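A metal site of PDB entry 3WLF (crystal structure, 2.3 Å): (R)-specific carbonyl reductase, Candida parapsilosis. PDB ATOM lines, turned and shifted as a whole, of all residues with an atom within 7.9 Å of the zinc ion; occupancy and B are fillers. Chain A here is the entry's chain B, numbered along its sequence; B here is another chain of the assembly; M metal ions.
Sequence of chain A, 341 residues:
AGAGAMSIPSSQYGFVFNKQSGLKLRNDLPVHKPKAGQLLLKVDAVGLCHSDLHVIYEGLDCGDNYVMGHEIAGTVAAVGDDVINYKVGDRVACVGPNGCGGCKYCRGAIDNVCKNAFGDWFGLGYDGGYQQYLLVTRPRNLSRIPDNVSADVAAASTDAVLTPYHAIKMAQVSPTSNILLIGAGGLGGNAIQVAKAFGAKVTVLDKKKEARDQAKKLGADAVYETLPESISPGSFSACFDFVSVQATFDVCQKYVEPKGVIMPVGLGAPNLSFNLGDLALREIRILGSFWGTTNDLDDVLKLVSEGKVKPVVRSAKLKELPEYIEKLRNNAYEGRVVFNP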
ATOM      1  N   ASN A  98     -14.316   4.996 -10.242  1.00  0.00           N
ATOM      2  CA  ASN A  98     -14.225   5.352  -8.827  1.00  0.00           C
ATOM      3  C   ASN A  98     -13.547   4.254  -7.998  1.00  0.00           C
ATOM      4  O   ASN A  98     -14.110   3.778  -7.015  1.00  0.00           O
ATOM      5  CB  ASN A  98     -15.634   5.626  -8.282  1.00  0.00           C
ATOM      6  CG  ASN A  98     -15.634   6.178  -6.880  1.00  0.00           C
ATOM      7  OD1 ASN A  98     -14.884   7.111  -6.555  1.00  0.00           O
ATOM      8  ND2 ASN A  98     -16.493   5.629  -6.019  1.00  0.00           N
ATOM      9  N   GLY A  99     -12.332   3.886  -8.400  1.00  0.00           N
ATOM     10  CA  GLY A  99     -11.590   2.848  -7.694  1.00  0.00           C
ATOM     11  C   GLY A  99     -11.394   3.089  -6.208  1.00  0.00           C
ATOM     12  O   GLY A  99     -11.392   4.237  -5.760  1.00  0.00           O
ATOM     13  N   CYS A 100     -11.226   2.017  -5.447  1.00  0.00           N
ATOM     14  CA  CYS A 100     -11.037   2.121  -4.006  1.00  0.00           C
ATOM     15  C   CYS A 100      -9.714   2.794  -3.670  1.00  0.00           C
ATOM     16  O   CYS A 100      -9.614   3.526  -2.682  1.00  0.00           O
ATOM     17  CB  CYS A 100     -11.084   0.728  -3.356  1.00  0.00           C
ATOM     18  SG  CYS A 100      -9.650  -0.328  -3.666  1.00  0.00           S
ATOM     19  N   GLY A 101      -8.706   2.553  -4.491  1.00  0.00           N
ATOM     20  CA  GLY A 101      -7.399   3.166  -4.275  1.00  0.00           C
ATOM     21  C   GLY A 101      -6.528   2.434  -3.268  1.00  0.00           C
ATOM     22  O   GLY A 101      -5.470   2.940  -2.888  1.00  0.00           O
ATOM     23  N   GLY A 102      -6.952   1.245  -2.842  1.00  0.00           N
ATOM     24  CA  GLY A 102      -6.177   0.499  -1.875  1.00  0.00           C
ATOM     25  C   GLY A 102      -5.756  -0.894  -2.303  1.00  0.00           C
ATOM     26  O   GLY A 102      -4.882  -1.499  -1.664  1.00  0.00           O
ATOM     27  N   CYS A 103      -6.356  -1.417  -3.364  1.00  0.00           N
ATOM     28  CA  CYS A 103      -6.011  -2.753  -3.842  1.00  0.00           C
ATOM     29  C   CYS A 103      -4.847  -2.707  -4.824  1.00  0.00           C
ATOM     30  O   CYS A 103      -4.443  -1.632  -5.267  1.00  0.00           O
ATOM     31  CB  CYS A 103      -7.228  -3.411  -4.496  1.00  0.00           C
ATOM     32  SG  CYS A 103      -7.807  -2.594  -6.000  1.00  0.00           S
ATOM     33  N   LYS A 104      -4.316  -3.874  -5.159  1.00  0.00           N
ATOM     34  CA  LYS A 104      -3.185  -3.963  -6.092  1.00  0.00           C
ATOM     35  C   LYS A 104      -3.541  -3.422  -7.477  1.00  0.00           C
ATOM     36  O   LYS A 104      -2.669  -2.948  -8.204  1.00  0.00           O
ATOM     37  CB  LYS A 104      -2.700  -5.409  -6.202  1.00  0.00           C
ATOM     38  CG  LYS A 104      -3.728  -6.385  -6.755  1.00  0.00           C
ATOM     39  CD  LYS A 104      -3.113  -7.761  -6.961  1.00  0.00           C
ATOM     40  CE  LYS A 104      -4.124  -8.746  -7.534  1.00  0.00           C
ATOM     41  NZ  LYS A 104      -3.510 -10.070  -7.833  1.00  0.00           N
ATOM     42  N   TYR A 105      -4.819  -3.508  -7.840  1.00  0.00           N
ATOM     43  CA  TYR A 105      -5.258  -3.021  -9.139  1.00  0.00           C
ATOM     44  C   TYR A 105      -5.193  -1.500  -9.190  1.00  0.00           C
ATOM     45  O   TYR A 105      -4.643  -0.922 -10.126  1.00  0.00           O
ATOM     46  CB  TYR A 105      -6.679  -3.502  -9.424  1.00  0.00           C
ATOM     47  CG  TYR A 105      -6.790  -5.016  -9.500  1.00  0.00           C
ATOM     48  CD1 TYR A 105      -6.201  -5.715 -10.547  1.00  0.00           C
ATOM     49  CD2 TYR A 105      -7.447  -5.729  -8.496  1.00  0.00           C
ATOM     50  CE1 TYR A 105      -6.276  -7.107 -10.597  1.00  0.00           C
ATOM     51  CE2 TYR A 105      -7.508  -7.125  -8.542  1.00  0.00           C
ATOM     52  CZ  TYR A 105      -6.926  -7.803  -9.595  1.00  0.00           C
ATOM     53  OH  TYR A 105      -6.987  -9.175  -9.643  1.00  0.00           O
ATOM     54  N   CYS A 106      -5.745  -0.845  -8.169  1.00  0.00           N
ATOM     55  CA  CYS A 106      -5.727   0.615  -8.102  1.00  0.00           C
ATOM     56  C   CYS A 106      -4.301   1.106  -7.925  1.00  0.00           C
ATOM     57  O   CYS A 106      -3.905   2.108  -8.513  1.00  0.00           O
ATOM     58  CB  CYS A 106      -6.596   1.103  -6.943  1.00  0.00           C
ATOM     59  SG  CYS A 106      -8.374   0.921  -7.192  1.00  0.00           S
ATOM     60  N   ARG A 107      -3.532   0.406  -7.100  1.00  0.00           N
ATOM     61  CA  ARG A 107      -2.140   0.780  -6.845  1.00  0.00           C
ATOM     62  C   ARG A 107      -1.236   0.320  -7.981  1.00  0.00           C
ATOM     63  O   ARG A 107      -0.044   0.662  -8.013  1.00  0.00           O
ATOM     64  CB  ARG A 107      -1.669   0.178  -5.522  1.00  0.00           C
ATOM     65  CG  ARG A 107      -2.262   0.867  -4.300  1.00  0.00           C
ATOM     66  CD  ARG A 107      -1.704   0.275  -3.010  1.00  0.00           C
ATOM     67  NE  ARG A 107      -2.329  -1.005  -2.680  1.00  0.00           N
ATOM     68  CZ  ARG A 107      -1.648  -2.098  -2.333  1.00  0.00           C
ATOM     69  NH1 ARG A 107      -0.328  -2.076  -2.263  1.00  0.00           N
ATOM     70  NH2 ARG A 107      -2.308  -3.216  -2.043  1.00  0.00           N
ATOM     71  N   ILE A 110      -4.239   0.575 -12.609  1.00  0.00           N
ATOM     72  CA  ILE A 110      -5.406   0.102 -13.343  1.00  0.00           C
ATOM     73  C   ILE A 110      -6.642   0.124 -12.451  1.00  0.00           C
ATOM     74  O   ILE A 110      -7.290  -0.902 -12.244  1.00  0.00           O
ATOM     75  CB  ILE A 110      -5.186  -1.312 -13.930  1.00  0.00           C
ATOM     76  CG1 ILE A 110      -4.857  -2.305 -12.810  1.00  0.00           C
ATOM     77  CG2 ILE A 110      -4.063  -1.283 -14.956  1.00  0.00           C
ATOM     78  CD1 ILE A 110      -4.614  -3.722 -13.299  1.00  0.00           C
ATOM     79  N   ASP A 111      -6.957   1.304 -11.932  1.00  0.00           N
ATOM     80  CA  ASP A 111      -8.104   1.464 -11.056  1.00  0.00           C
ATOM     81  C   ASP A 111      -9.444   1.307 -11.762  1.00  0.00           C
ATOM     82  O   ASP A 111     -10.493   1.356 -11.120  1.00  0.00           O
ATOM     83  CB  ASP A 111      -8.048   2.836 -10.365  1.00  0.00           C
ATOM     84  CG  ASP A 111      -7.791   3.964 -11.337  1.00  0.00           C
ATOM     85  OD1 ASP A 111      -8.271   3.894 -12.485  1.00  0.00           O
ATOM     86  OD2 ASP A 111      -7.117   4.946 -10.942  1.00  0.00           O
ATOM     87  N   ASN A 112      -9.420   1.108 -13.074  1.00  0.00           N
ATOM     88  CA  ASN A 112     -10.643   0.938 -13.846  1.00  0.00           C
ATOM     89  C   ASN A 112     -11.228  -0.471 -13.721  1.00  0.00           C
ATOM     90  O   ASN A 112     -12.365  -0.713 -14.128  1.00  0.00           O
ATOM     91  CB  ASN A 112     -10.399   1.276 -15.323  1.00  0.00           C
ATOM     92  CG  ASN A 112      -9.378   0.353 -15.977  1.00  0.00           C
ATOM     93  OD1 ASN A 112      -8.268   0.197 -15.474  1.00  0.00           O
ATOM     94  ND2 ASN A 112      -9.754  -0.249 -17.102  1.00  0.00           N
ATOM     95  N   VAL A 113     -10.452  -1.401 -13.176  1.00  0.00           N
ATOM     96  CA  VAL A 113     -10.911  -2.767 -13.001  1.00  0.00           C
ATOM     97  C   VAL A 113     -10.877  -3.162 -11.526  1.00  0.00           C
ATOM     98  O   VAL A 113     -10.722  -4.344 -11.186  1.00  0.00           O
ATOM     99  CB  VAL A 113     -10.053  -3.786 -13.795  1.00  0.00           C
ATOM    100  CG1 VAL A 113     -10.182  -3.503 -15.290  1.00  0.00           C
ATOM    101  CG2 VAL A 113      -8.599  -3.715 -13.353  1.00  0.00           C
ATOM    102  N   CYS A 114     -11.028  -2.184 -10.644  1.00  0.00           N
ATOM    103  CA  CYS A 114     -11.031  -2.429  -9.215  1.00  0.00           C
ATOM    104  C   CYS A 114     -12.233  -3.286  -8.833  1.00  0.00           C
ATOM    105  O   CYS A 114     -13.378  -2.940  -9.127  1.00  0.00           O
ATOM    106  CB  CYS A 114     -11.076  -1.106  -8.455  1.00  0.00           C
ATOM    107  SG  CYS A 114     -11.240  -1.274  -6.668  1.00  0.00           S
ATOM    108  N   LYS A 115     -11.965  -4.421  -8.175  1.00  0.00           N
ATOM    109  CA  LYS A 115     -13.040  -5.314  -7.763  1.00  0.00           C
ATOM    110  C   LYS A 115     -13.869  -4.727  -6.630  1.00  0.00           C
ATOM    111  O   LYS A 115     -15.099  -4.796  -6.664  1.00  0.00           O
ATOM    112  CB  LYS A 115     -12.462  -6.663  -7.316  1.00  0.00           C
ATOM    113  CG  LYS A 115     -11.835  -7.479  -8.440  1.00  0.00           C
ATOM    114  CD  LYS A 115     -11.324  -8.821  -7.923  1.00  0.00           C
ATOM    115  CE  LYS A 115     -10.714  -9.660  -9.040  1.00  0.00           C
ATOM    116  NZ  LYS A 115     -10.216 -10.970  -8.549  1.00  0.00           N
ATOM    117  N   ASN A 116     -13.206  -4.153  -5.639  1.00  0.00           N
ATOM    118  CA  ASN A 116     -13.894  -3.567  -4.490  1.00  0.00           C
ATOM    119  C   ASN A 116     -14.827  -2.435  -4.911  1.00  0.00           C
ATOM    120  O   ASN A 116     -15.842  -2.182  -4.246  1.00  0.00           O
ATOM    121  CB  ASN A 116     -12.884  -3.014  -3.476  1.00  0.00           C
ATOM    122  CG  ASN A 116     -11.948  -4.082  -2.939  1.00  0.00           C
ATOM    123  OD1 ASN A 116     -12.379  -5.172  -2.567  1.00  0.00           O
ATOM    124  ND2 ASN A 116     -10.662  -3.757  -2.898  1.00  0.00           N
ATOM    125  N   ALA A 117     -14.492  -1.759  -5.998  1.00  0.00           N
ATOM    126  CA  ALA A 117     -15.292  -0.631  -6.475  1.00  0.00           C
ATOM    127  C   ALA A 117     -16.436  -1.022  -7.395  1.00  0.00           C
ATOM    128  O   ALA A 117     -17.299  -0.197  -7.707  1.00  0.00           O
ATOM    129  CB  ALA A 117     -14.383   0.391  -7.178  1.00  0.00           C
ATOM    130  N   PHE A 118     -16.463  -2.266  -7.845  1.00  0.00           N
ATOM    131  CA  PHE A 118     -17.540  -2.706  -8.726  1.00  0.00           C
ATOM    132  C   PHE A 118     -18.867  -2.595  -7.978  1.00  0.00           C
ATOM    133  O   PHE A 118     -19.042  -3.206  -6.922  1.00  0.00           O
ATOM    134  CB  PHE A 118     -17.306  -4.143  -9.204  1.00  0.00           C
ATOM    135  CG  PHE A 118     -18.301  -4.600 -10.243  1.00  0.00           C
ATOM    136  CD1 PHE A 118     -19.571  -5.037  -9.869  1.00  0.00           C
ATOM    137  CD2 PHE A 118     -17.974  -4.565 -11.595  1.00  0.00           C
ATOM    138  CE1 PHE A 118     -20.507  -5.426 -10.828  1.00  0.00           C
ATOM    139  CE2 PHE A 118     -18.907  -4.950 -12.562  1.00  0.00           C
ATOM    140  CZ  PHE A 118     -20.172  -5.387 -12.175  1.00  0.00           C
ATOM    141  N   ARG A 138     -13.958   9.422  -2.522  1.00  0.00           N
ATOM    142  CA  ARG A 138     -12.542   9.232  -2.794  1.00  0.00           C
ATOM    143  C   ARG A 138     -12.034  10.228  -3.831  1.00  0.00           C
ATOM    144  O   ARG A 138     -12.101   9.989  -5.033  1.00  0.00           O
ATOM    145  CB  ARG A 138     -12.288   7.795  -3.265  1.00  0.00           C
ATOM    146  CG  ARG A 138     -12.665   6.746  -2.214  1.00  0.00           C
ATOM    147  CD  ARG A 138     -12.258   5.342  -2.628  1.00  0.00           C
ATOM    148  NE  ARG A 138     -13.110   4.769  -3.663  1.00  0.00           N
ATOM    149  CZ  ARG A 138     -14.374   4.391  -3.467  1.00  0.00           C
ATOM    150  NH1 ARG A 138     -15.075   3.879  -4.469  1.00  0.00           N
ATOM    151  NH2 ARG A 138     -14.943   4.509  -2.267  1.00  0.00           N
ATOM    152  N   ARG A 140      -9.327  10.883  -4.978  1.00  0.00           N
ATOM    153  CA  ARG A 140      -8.285  10.395  -5.885  1.00  0.00           C
ATOM    154  C   ARG A 140      -8.873  10.232  -7.275  1.00  0.00           C
ATOM    155  O   ARG A 140      -8.177  10.366  -8.276  1.00  0.00           O
ATOM    156  CB  ARG A 140      -7.719   9.056  -5.403  1.00  0.00           C
ATOM    157  CG  ARG A 140      -8.646   7.861  -5.644  1.00  0.00           C
ATOM    158  CD  ARG A 140      -8.014   6.544  -5.188  1.00  0.00           C
ATOM    159  NE  ARG A 140      -6.876   6.121  -6.012  1.00  0.00           N
ATOM    160  CZ  ARG A 140      -6.977   5.669  -7.253  1.00  0.00           C
ATOM    161  NH1 ARG A 140      -5.883   5.310  -7.920  1.00  0.00           N
ATOM    162  NH2 ARG A 140      -8.161   5.573  -7.845  1.00  0.00           N
ATOM    163  N   ASN B  85     -11.594  -2.342   3.902  1.00  0.00           N
ATOM    164  CA  ASN B  85     -10.554  -3.203   3.359  1.00  0.00           C
ATOM    165  C   ASN B  85      -9.698  -3.830   4.458  1.00  0.00           C
ATOM    166  O   ASN B  85      -8.891  -4.726   4.191  1.00  0.00           O
ATOM    167  CB  ASN B  85      -9.677  -2.424   2.391  1.00  0.00           C
ATOM    168  CG  ASN B  85     -10.437  -1.930   1.172  1.00  0.00           C
ATOM    169  OD1 ASN B  85     -11.062  -2.707   0.455  1.00  0.00           O
ATOM    170  ND2 ASN B  85     -10.395  -0.615   0.943  1.00  0.00           N
HETATM  171 ZN    ZN M   1      -9.183  -0.826  -5.854  1.00  0.00          ZN
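Gly 101 touches the zinc ion. Five residues have an atom within 4 Å of the zinc ion: Cys 100, Gly 101, Cys 103, Cys 106 and Cys 114. The nearest printed residue that does not touch the zinc ion is Gly 102 (4.3 Å).
The zinc ion is bound by SG of Cys 103, SG of Cys 114, SG of Cys 100 and SG of Cys 106.
The backbone NH (N) of Tyr 105 sits close to the side-chain sulfur (SG) of Cys 103, at 3.6 Å. The backbone carbonyl oxygen (O) of Cys 103 lies close to the guanidinium group (NE) of Arg 107 (3.4 Å). SG of Cys 114 lies close to N of Asn 116 (3.6 Å). The side-chain sulfur of Cys 114 lies close to the backbone NH of Ala 117 (3.4 Å). The side-chain sulfur of Cys 100 lies close to the backbone NH of Gly 102 (3.2 Å). The side-chain sulfur of Cys 100 sits close to the side-chain amide nitrogen of Asn 116 (3.7 Å). The backbone NH of Gly 101 lies close to the side-chain sulfur of Cys 106.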
